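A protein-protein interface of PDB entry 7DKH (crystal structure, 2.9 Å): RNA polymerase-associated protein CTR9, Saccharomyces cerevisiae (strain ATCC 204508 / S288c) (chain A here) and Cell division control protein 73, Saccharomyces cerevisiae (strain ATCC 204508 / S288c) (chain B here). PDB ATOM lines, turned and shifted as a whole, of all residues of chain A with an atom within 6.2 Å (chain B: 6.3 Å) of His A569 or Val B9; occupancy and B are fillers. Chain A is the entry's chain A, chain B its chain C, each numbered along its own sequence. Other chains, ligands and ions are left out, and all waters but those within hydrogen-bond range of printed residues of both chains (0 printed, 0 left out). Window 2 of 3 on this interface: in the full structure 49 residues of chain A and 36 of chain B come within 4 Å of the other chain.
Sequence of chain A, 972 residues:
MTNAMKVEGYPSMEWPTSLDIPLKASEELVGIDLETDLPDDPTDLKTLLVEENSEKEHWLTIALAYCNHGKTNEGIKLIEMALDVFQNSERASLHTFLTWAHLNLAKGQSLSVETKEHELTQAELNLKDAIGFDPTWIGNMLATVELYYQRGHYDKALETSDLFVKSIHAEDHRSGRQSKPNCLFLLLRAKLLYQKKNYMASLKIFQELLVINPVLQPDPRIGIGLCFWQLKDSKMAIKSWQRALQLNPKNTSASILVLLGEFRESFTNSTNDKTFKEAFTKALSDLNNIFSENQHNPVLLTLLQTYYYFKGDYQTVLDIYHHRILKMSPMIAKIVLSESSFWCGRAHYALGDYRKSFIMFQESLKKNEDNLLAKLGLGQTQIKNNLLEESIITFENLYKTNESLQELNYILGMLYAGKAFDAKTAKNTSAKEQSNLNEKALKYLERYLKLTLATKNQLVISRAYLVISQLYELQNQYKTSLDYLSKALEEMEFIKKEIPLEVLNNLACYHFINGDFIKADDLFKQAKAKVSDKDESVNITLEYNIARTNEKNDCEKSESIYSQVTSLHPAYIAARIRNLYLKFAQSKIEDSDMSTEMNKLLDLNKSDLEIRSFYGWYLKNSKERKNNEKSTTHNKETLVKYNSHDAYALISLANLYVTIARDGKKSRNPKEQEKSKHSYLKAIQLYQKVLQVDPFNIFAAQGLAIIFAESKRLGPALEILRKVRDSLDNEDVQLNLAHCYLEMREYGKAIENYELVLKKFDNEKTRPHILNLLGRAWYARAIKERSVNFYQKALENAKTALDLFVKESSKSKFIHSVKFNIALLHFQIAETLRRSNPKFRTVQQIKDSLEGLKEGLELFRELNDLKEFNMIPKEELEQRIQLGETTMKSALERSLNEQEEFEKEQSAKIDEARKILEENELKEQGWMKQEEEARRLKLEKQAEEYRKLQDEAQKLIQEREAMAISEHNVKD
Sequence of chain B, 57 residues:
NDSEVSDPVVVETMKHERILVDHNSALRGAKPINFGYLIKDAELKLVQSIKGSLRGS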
ATOM      1  N   GLU A 536       3.428 -17.122 -26.548  1.00  0.00           N
ATOM      2  CA  GLU A 536       2.992 -15.761 -26.236  1.00  0.00           C
ATOM      3  C   GLU A 536       1.976 -15.684 -25.099  1.00  0.00           C
ATOM      4  O   GLU A 536       1.776 -14.590 -24.551  1.00  0.00           O
ATOM      5  CB  GLU A 536       2.352 -15.099 -27.464  1.00  0.00           C
ATOM      6  CG  GLU A 536       3.307 -14.440 -28.434  1.00  0.00           C
ATOM      7  CD  GLU A 536       4.078 -15.451 -29.248  1.00  0.00           C
ATOM      8  OE1 GLU A 536       3.518 -16.531 -29.540  1.00  0.00           O
ATOM      9  OE2 GLU A 536       5.244 -15.171 -29.593  1.00  0.00           O
ATOM     10  N   SER A 537       1.378 -16.807 -24.686  1.00  0.00           N
ATOM     11  CA  SER A 537       0.488 -16.791 -23.528  1.00  0.00           C
ATOM     12  C   SER A 537       1.227 -16.370 -22.263  1.00  0.00           C
ATOM     13  O   SER A 537       0.810 -15.435 -21.571  1.00  0.00           O
ATOM     14  CB  SER A 537      -0.168 -18.159 -23.349  1.00  0.00           C
ATOM     15  OG  SER A 537       0.735 -19.206 -23.656  1.00  0.00           O
ATOM     16  N   ILE A 540       2.860 -12.669 -22.553  1.00  0.00           N
ATOM     17  CA  ILE A 540       2.031 -11.497 -22.257  1.00  0.00           C
ATOM     18  C   ILE A 540       2.096 -11.146 -20.774  1.00  0.00           C
ATOM     19  O   ILE A 540       2.296  -9.981 -20.399  1.00  0.00           O
ATOM     20  CB  ILE A 540       0.571 -11.751 -22.678  1.00  0.00           C
ATOM     21  CG1 ILE A 540       0.423 -11.802 -24.191  1.00  0.00           C
ATOM     22  CG2 ILE A 540      -0.357 -10.695 -22.080  1.00  0.00           C
ATOM     23  CD1 ILE A 540      -1.000 -12.055 -24.619  1.00  0.00           C
ATOM     24  N   GLN A 564       2.038  -1.893 -26.493  1.00  0.00           N
ATOM     25  CA  GLN A 564       2.112  -3.103 -27.307  1.00  0.00           C
ATOM     26  C   GLN A 564       1.051  -4.113 -26.883  1.00  0.00           C
ATOM     27  O   GLN A 564       0.359  -4.697 -27.732  1.00  0.00           O
ATOM     28  CB  GLN A 564       3.498  -3.746 -27.202  1.00  0.00           C
ATOM     29  CG  GLN A 564       4.645  -3.034 -27.888  1.00  0.00           C
ATOM     30  CD  GLN A 564       5.867  -3.934 -27.984  1.00  0.00           C
ATOM     31  OE1 GLN A 564       5.753  -5.157 -27.905  1.00  0.00           O
ATOM     32  NE2 GLN A 564       7.045  -3.332 -28.117  1.00  0.00           N
ATOM     33  N   VAL A 565       0.870  -4.295 -25.569  1.00  0.00           N
ATOM     34  CA  VAL A 565      -0.103  -5.279 -25.096  1.00  0.00           C
ATOM     35  C   VAL A 565      -1.533  -4.808 -25.338  1.00  0.00           C
ATOM     36  O   VAL A 565      -2.427  -5.625 -25.585  1.00  0.00           O
ATOM     37  CB  VAL A 565       0.145  -5.603 -23.608  1.00  0.00           C
ATOM     38  CG1 VAL A 565      -0.905  -6.565 -23.072  1.00  0.00           C
ATOM     39  CG2 VAL A 565       1.524  -6.201 -23.423  1.00  0.00           C
ATOM     40  N   THR A 566      -1.773  -3.497 -25.328  1.00  0.00           N
ATOM     41  CA  THR A 566      -3.131  -3.013 -25.539  1.00  0.00           C
ATOM     42  C   THR A 566      -3.488  -2.984 -27.020  1.00  0.00           C
ATOM     43  O   THR A 566      -4.651  -3.185 -27.384  1.00  0.00           O
ATOM     44  CB  THR A 566      -3.294  -1.624 -24.927  1.00  0.00           C
ATOM     45  OG1 THR A 566      -2.176  -0.809 -25.298  1.00  0.00           O
ATOM     46  CG2 THR A 566      -3.351  -1.724 -23.407  1.00  0.00           C
ATOM     47  N   SER A 567      -2.503  -2.721 -27.885  1.00  0.00           N
ATOM     48  CA  SER A 567      -2.730  -2.799 -29.322  1.00  0.00           C
ATOM     49  C   SER A 567      -2.961  -4.236 -29.771  1.00  0.00           C
ATOM     50  O   SER A 567      -3.957  -4.534 -30.441  1.00  0.00           O
ATOM     51  CB  SER A 567      -1.541  -2.194 -30.067  1.00  0.00           C
ATOM     52  OG  SER A 567      -0.614  -3.202 -30.435  1.00  0.00           O
ATOM     53  N   LEU A 568      -2.060  -5.151 -29.398  1.00  0.00           N
ATOM     54  CA  LEU A 568      -2.159  -6.510 -29.921  1.00  0.00           C
ATOM     55  C   LEU A 568      -3.285  -7.281 -29.237  1.00  0.00           C
ATOM     56  O   LEU A 568      -4.140  -7.875 -29.905  1.00  0.00           O
ATOM     57  CB  LEU A 568      -0.821  -7.237 -29.768  1.00  0.00           C
ATOM     58  CG  LEU A 568      -0.703  -8.552 -30.544  1.00  0.00           C
ATOM     59  CD1 LEU A 568      -1.487  -8.471 -31.852  1.00  0.00           C
ATOM     60  CD2 LEU A 568       0.752  -8.889 -30.834  1.00  0.00           C
ATOM     61  N   HIS A 569      -3.310  -7.275 -27.902  1.00  0.00           N
ATOM     62  CA  HIS A 569      -4.268  -8.049 -27.113  1.00  0.00           C
ATOM     63  C   HIS A 569      -5.070  -7.091 -26.238  1.00  0.00           C
ATOM     64  O   HIS A 569      -4.801  -6.955 -25.034  1.00  0.00           O
ATOM     65  CB  HIS A 569      -3.553  -9.104 -26.273  1.00  0.00           C
ATOM     66  CG  HIS A 569      -2.659 -10.002 -27.067  1.00  0.00           C
ATOM     67  ND1 HIS A 569      -3.141 -11.016 -27.866  1.00  0.00           N
ATOM     68  CD2 HIS A 569      -1.313 -10.032 -27.196  1.00  0.00           C
ATOM     69  CE1 HIS A 569      -2.131 -11.637 -28.445  1.00  0.00           C
ATOM     70  NE2 HIS A 569      -1.010 -11.061 -28.053  1.00  0.00           N
ATOM     71  N   PRO A 570      -6.068  -6.413 -26.811  1.00  0.00           N
ATOM     72  CA  PRO A 570      -6.854  -5.452 -26.021  1.00  0.00           C
ATOM     73  C   PRO A 570      -7.657  -6.091 -24.905  1.00  0.00           C
ATOM     74  O   PRO A 570      -8.074  -5.378 -23.985  1.00  0.00           O
ATOM     75  CB  PRO A 570      -7.769  -4.796 -27.066  1.00  0.00           C
ATOM     76  CG  PRO A 570      -7.243  -5.236 -28.407  1.00  0.00           C
ATOM     77  CD  PRO A 570      -6.577  -6.547 -28.181  1.00  0.00           C
ATOM     78  N   ALA A 571      -7.890  -7.404 -24.947  1.00  0.00           N
ATOM     79  CA  ALA A 571      -8.673  -8.051 -23.902  1.00  0.00           C
ATOM     80  C   ALA A 571      -7.902  -8.186 -22.597  1.00  0.00           C
ATOM     81  O   ALA A 571      -8.519  -8.449 -21.560  1.00  0.00           O
ATOM     82  CB  ALA A 571      -9.154  -9.429 -24.366  1.00  0.00           C
ATOM     83  N   TYR A 572      -6.583  -8.005 -22.617  1.00  0.00           N
ATOM     84  CA  TYR A 572      -5.783  -8.035 -21.396  1.00  0.00           C
ATOM     85  C   TYR A 572      -6.027  -6.752 -20.605  1.00  0.00           C
ATOM     86  O   TYR A 572      -5.571  -5.673 -20.993  1.00  0.00           O
ATOM     87  CB  TYR A 572      -4.304  -8.211 -21.725  1.00  0.00           C
ATOM     88  CG  TYR A 572      -3.506  -8.704 -20.547  1.00  0.00           C
ATOM     89  CD1 TYR A 572      -3.609 -10.020 -20.113  1.00  0.00           C
ATOM     90  CD2 TYR A 572      -2.668  -7.846 -19.848  1.00  0.00           C
ATOM     91  CE1 TYR A 572      -2.885 -10.473 -19.021  1.00  0.00           C
ATOM     92  CE2 TYR A 572      -1.944  -8.287 -18.758  1.00  0.00           C
ATOM     93  CZ  TYR A 572      -2.054  -9.599 -18.347  1.00  0.00           C
ATOM     94  OH  TYR A 572      -1.329 -10.032 -17.262  1.00  0.00           O
ATOM     95  N   ILE A 573      -6.735  -6.880 -19.482  1.00  0.00           N
ATOM     96  CA  ILE A 573      -7.372  -5.729 -18.847  1.00  0.00           C
ATOM     97  C   ILE A 573      -6.362  -4.880 -18.082  1.00  0.00           C
ATOM     98  O   ILE A 573      -6.398  -3.643 -18.142  1.00  0.00           O
ATOM     99  CB  ILE A 573      -8.501  -6.216 -17.923  1.00  0.00           C
ATOM    100  CG1 ILE A 573      -9.546  -6.976 -18.742  1.00  0.00           C
ATOM    101  CG2 ILE A 573      -9.106  -5.061 -17.165  1.00  0.00           C
ATOM    102  CD1 ILE A 573     -10.231  -6.116 -19.769  1.00  0.00           C
ATOM    103  N   ALA A 575      -3.201  -4.238 -18.459  1.00  0.00           N
ATOM    104  CA  ALA A 575      -2.413  -3.347 -19.302  1.00  0.00           C
ATOM    105  C   ALA A 575      -3.212  -2.116 -19.710  1.00  0.00           C
ATOM    106  O   ALA A 575      -2.688  -1.000 -19.683  1.00  0.00           O
ATOM    107  CB  ALA A 575      -1.915  -4.093 -20.539  1.00  0.00           C
ATOM    108  N   ARG A 576      -4.481  -2.301 -20.085  1.00  0.00           N
ATOM    109  CA  ARG A 576      -5.316  -1.165 -20.472  1.00  0.00           C
ATOM    110  C   ARG A 576      -5.511  -0.204 -19.306  1.00  0.00           C
ATOM    111  O   ARG A 576      -5.361   1.019 -19.454  1.00  0.00           O
ATOM    112  CB  ARG A 576      -6.670  -1.652 -20.982  1.00  0.00           C
ATOM    113  CG  ARG A 576      -6.623  -2.487 -22.244  1.00  0.00           C
ATOM    114  CD  ARG A 576      -8.000  -2.555 -22.894  1.00  0.00           C
ATOM    115  NE  ARG A 576      -8.517  -1.240 -23.229  1.00  0.00           N
ATOM    116  CZ  ARG A 576      -9.655  -1.022 -23.878  1.00  0.00           C
ATOM    117  NH1 ARG A 576     -10.414  -2.036 -24.267  1.00  0.00           N
ATOM    118  NH2 ARG A 576     -10.039   0.222 -24.139  1.00  0.00           N
ATOM    119  N   ASP B   7     -10.221 -13.163 -27.884  1.00  0.00           N
ATOM    120  CA  ASP B   7      -8.780 -13.384 -28.008  1.00  0.00           C
ATOM    121  C   ASP B   7      -8.400 -14.700 -27.348  1.00  0.00           C
ATOM    122  O   ASP B   7      -8.359 -14.771 -26.103  1.00  0.00           O
ATOM    123  CB  ASP B   7      -8.015 -12.223 -27.375  1.00  0.00           C
ATOM    124  CG  ASP B   7      -6.610 -12.083 -27.915  1.00  0.00           C
ATOM    125  OD1 ASP B   7      -6.081 -13.068 -28.463  1.00  0.00           O
ATOM    126  OD2 ASP B   7      -6.036 -10.982 -27.781  1.00  0.00           O
ATOM    127  N   PRO B   8      -8.119 -15.761 -28.107  1.00  0.00           N
ATOM    128  CA  PRO B   8      -7.789 -17.047 -27.472  1.00  0.00           C
ATOM    129  C   PRO B   8      -6.479 -17.033 -26.700  1.00  0.00           C
ATOM    130  O   PRO B   8      -6.322 -17.842 -25.776  1.00  0.00           O
ATOM    131  CB  PRO B   8      -7.726 -18.026 -28.658  1.00  0.00           C
ATOM    132  CG  PRO B   8      -8.383 -17.308 -29.807  1.00  0.00           C
ATOM    133  CD  PRO B   8      -8.121 -15.855 -29.576  1.00  0.00           C
ATOM    134  N   VAL B   9      -5.543 -16.140 -27.033  1.00  0.00           N
ATOM    135  CA  VAL B   9      -4.223 -16.178 -26.405  1.00  0.00           C
ATOM    136  C   VAL B   9      -4.224 -15.495 -25.041  1.00  0.00           C
ATOM    137  O   VAL B   9      -3.452 -15.874 -24.150  1.00  0.00           O
ATOM    138  CB  VAL B   9      -3.188 -15.535 -27.348  1.00  0.00           C
ATOM    139  CG1 VAL B   9      -1.920 -15.125 -26.601  1.00  0.00           C
ATOM    140  CG2 VAL B   9      -2.856 -16.473 -28.493  1.00  0.00           C
ATOM    141  N   VAL B  10      -5.116 -14.530 -24.823  1.00  0.00           N
ATOM    142  CA  VAL B  10      -5.279 -14.011 -23.471  1.00  0.00           C
ATOM    143  C   VAL B  10      -6.168 -14.924 -22.640  1.00  0.00           C
ATOM    144  O   VAL B  10      -6.014 -14.986 -21.417  1.00  0.00           O
ATOM    145  CB  VAL B  10      -5.814 -12.567 -23.488  1.00  0.00           C
ATOM    146  CG1 VAL B  10      -5.033 -11.744 -24.489  1.00  0.00           C
ATOM    147  CG2 VAL B  10      -7.299 -12.537 -23.818  1.00  0.00           C
ATOM    148  N   VAL B  11      -7.089 -15.657 -23.278  1.00  0.00           N
ATOM    149  CA  VAL B  11      -7.908 -16.629 -22.553  1.00  0.00           C
ATOM    150  C   VAL B  11      -7.024 -17.653 -21.856  1.00  0.00           C
ATOM    151  O   VAL B  11      -7.240 -17.994 -20.686  1.00  0.00           O
ATOM    152  CB  VAL B  11      -8.913 -17.312 -23.501  1.00  0.00           C
ATOM    153  CG1 VAL B  11      -9.523 -18.536 -22.828  1.00  0.00           C
ATOM    154  CG2 VAL B  11     -10.018 -16.346 -23.886  1.00  0.00           C
ATOM    155  N   GLU B  12      -6.023 -18.169 -22.566  1.00  0.00           N
ATOM    156  CA  GLU B  12      -5.096 -19.099 -21.938  1.00  0.00           C
ATOM    157  C   GLU B  12      -4.073 -18.406 -21.047  1.00  0.00           C
ATOM    158  O   GLU B  12      -3.381 -19.087 -20.283  1.00  0.00           O
ATOM    159  CB  GLU B  12      -4.372 -19.937 -22.994  1.00  0.00           C
ATOM    160  CG  GLU B  12      -4.032 -21.332 -22.488  1.00  0.00           C
ATOM    161  CD  GLU B  12      -2.823 -21.935 -23.168  1.00  0.00           C
ATOM    162  OE1 GLU B  12      -1.841 -21.200 -23.401  1.00  0.00           O
ATOM    163  OE2 GLU B  12      -2.860 -23.146 -23.473  1.00  0.00           O
ATOM    164  N   THR B  13      -3.957 -17.076 -21.111  1.00  0.00           N
ATOM    165  CA  THR B  13      -3.139 -16.384 -20.120  1.00  0.00           C
ATOM    166  C   THR B  13      -3.834 -16.319 -18.764  1.00  0.00           C
ATOM    167  O   THR B  13      -3.195 -16.542 -17.730  1.00  0.00           O
ATOM    168  CB  THR B  13      -2.774 -14.977 -20.601  1.00  0.00           C
ATOM    169  OG1 THR B  13      -2.415 -15.019 -21.987  1.00  0.00           O
ATOM    170  CG2 THR B  13      -1.619 -14.414 -19.775  1.00  0.00           C
ATOM    171  N   MET B  14      -5.132 -16.020 -18.742  1.00  0.00           N
ATOM    172  CA  MET B  14      -5.886 -16.000 -17.487  1.00  0.00           C
ATOM    173  C   MET B  14      -5.913 -17.368 -16.805  1.00  0.00           C
ATOM    174  O   MET B  14      -5.883 -17.440 -15.579  1.00  0.00           O
ATOM    175  CB  MET B  14      -7.318 -15.506 -17.707  1.00  0.00           C
ATOM    176  CG  MET B  14      -7.488 -14.554 -18.866  1.00  0.00           C
ATOM    177  SD  MET B  14      -6.859 -12.763 -18.427  1.00  0.00           S
ATOM    178  CE  MET B  14      -8.448 -12.115 -17.503  1.00  0.00           C
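Of chain B, only Asp B7 (2.9 Å), Val B9 (3.95 Å) and Val B10 (3.5 Å) come within 4 Å of His A569. Val B9 touches just these residues of chain A: Ile A540 (3.8 Å) and His A569 (3.95 Å). Of the printed residues of chain A, Asp B7 touches His A569 (2.9 Å). Of the printed residues of chain A, Val B10 touches His A569 (3.5 Å) and Ala A571 (3.7 Å). Of the printed residues of chain B, Ser A537 touches Glu B12 and Thr B13. Of the printed residues of chain B, Ala A571 touches Val B10. Met B14 touches none of the printed residues of chain A. Val B11 touches none of the printed residues of chain A. The nearest printed residue of chain B that does not touch His A569 is Pro B8 (6.9 Å).
CG1 of Val B9 touches CD1 of Ile A540, at 3.8 Å. Val B9 touches His A569. His A569 touches Val B10. CG2 of Val B10 touches CB of Ala A571, 3.7 Å away.
The side-chain carboxylate (OD1) of Asp B7 lies close to the backbone NH (N) of Val B9 (3.4 Å). O of Val B9 is in hydrogen-bond range of OG1 of Thr B13 (2.5 Å).
Printed residues of chain A that touch a printed residue of chain B: Ser A537, Ile A540, His A569 and Ala A571. Of the 8 printed residues of chain B, 5 touch a printed residue of chain A. Printed residues of chain B that touch a printed residue of chain A: Asp B7, Val B9, Val B10, Glu B12 and Thr B13. Hydrophobic or aromatic side chains of chain B within 4 Å of the printed part of chain A: Val B9 and Val B10. Along chain B the printed residues that touch a printed residue of chain A span positions 7 to 13.
The backbone carbonyl oxygen (O) of Ser A537 sits close to the side-chain hydroxyl (OG1) of Thr B13, 3.3 Å away. A ring nitrogen (ND1) of His A569 lies within hydrogen-bond range of the side-chain carboxylate (OD2) of Asp B7 (2.9 Å). OG of Ser A537 lies within hydrogen-bond range of OE1 of Glu B12, 3.3 Å away.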
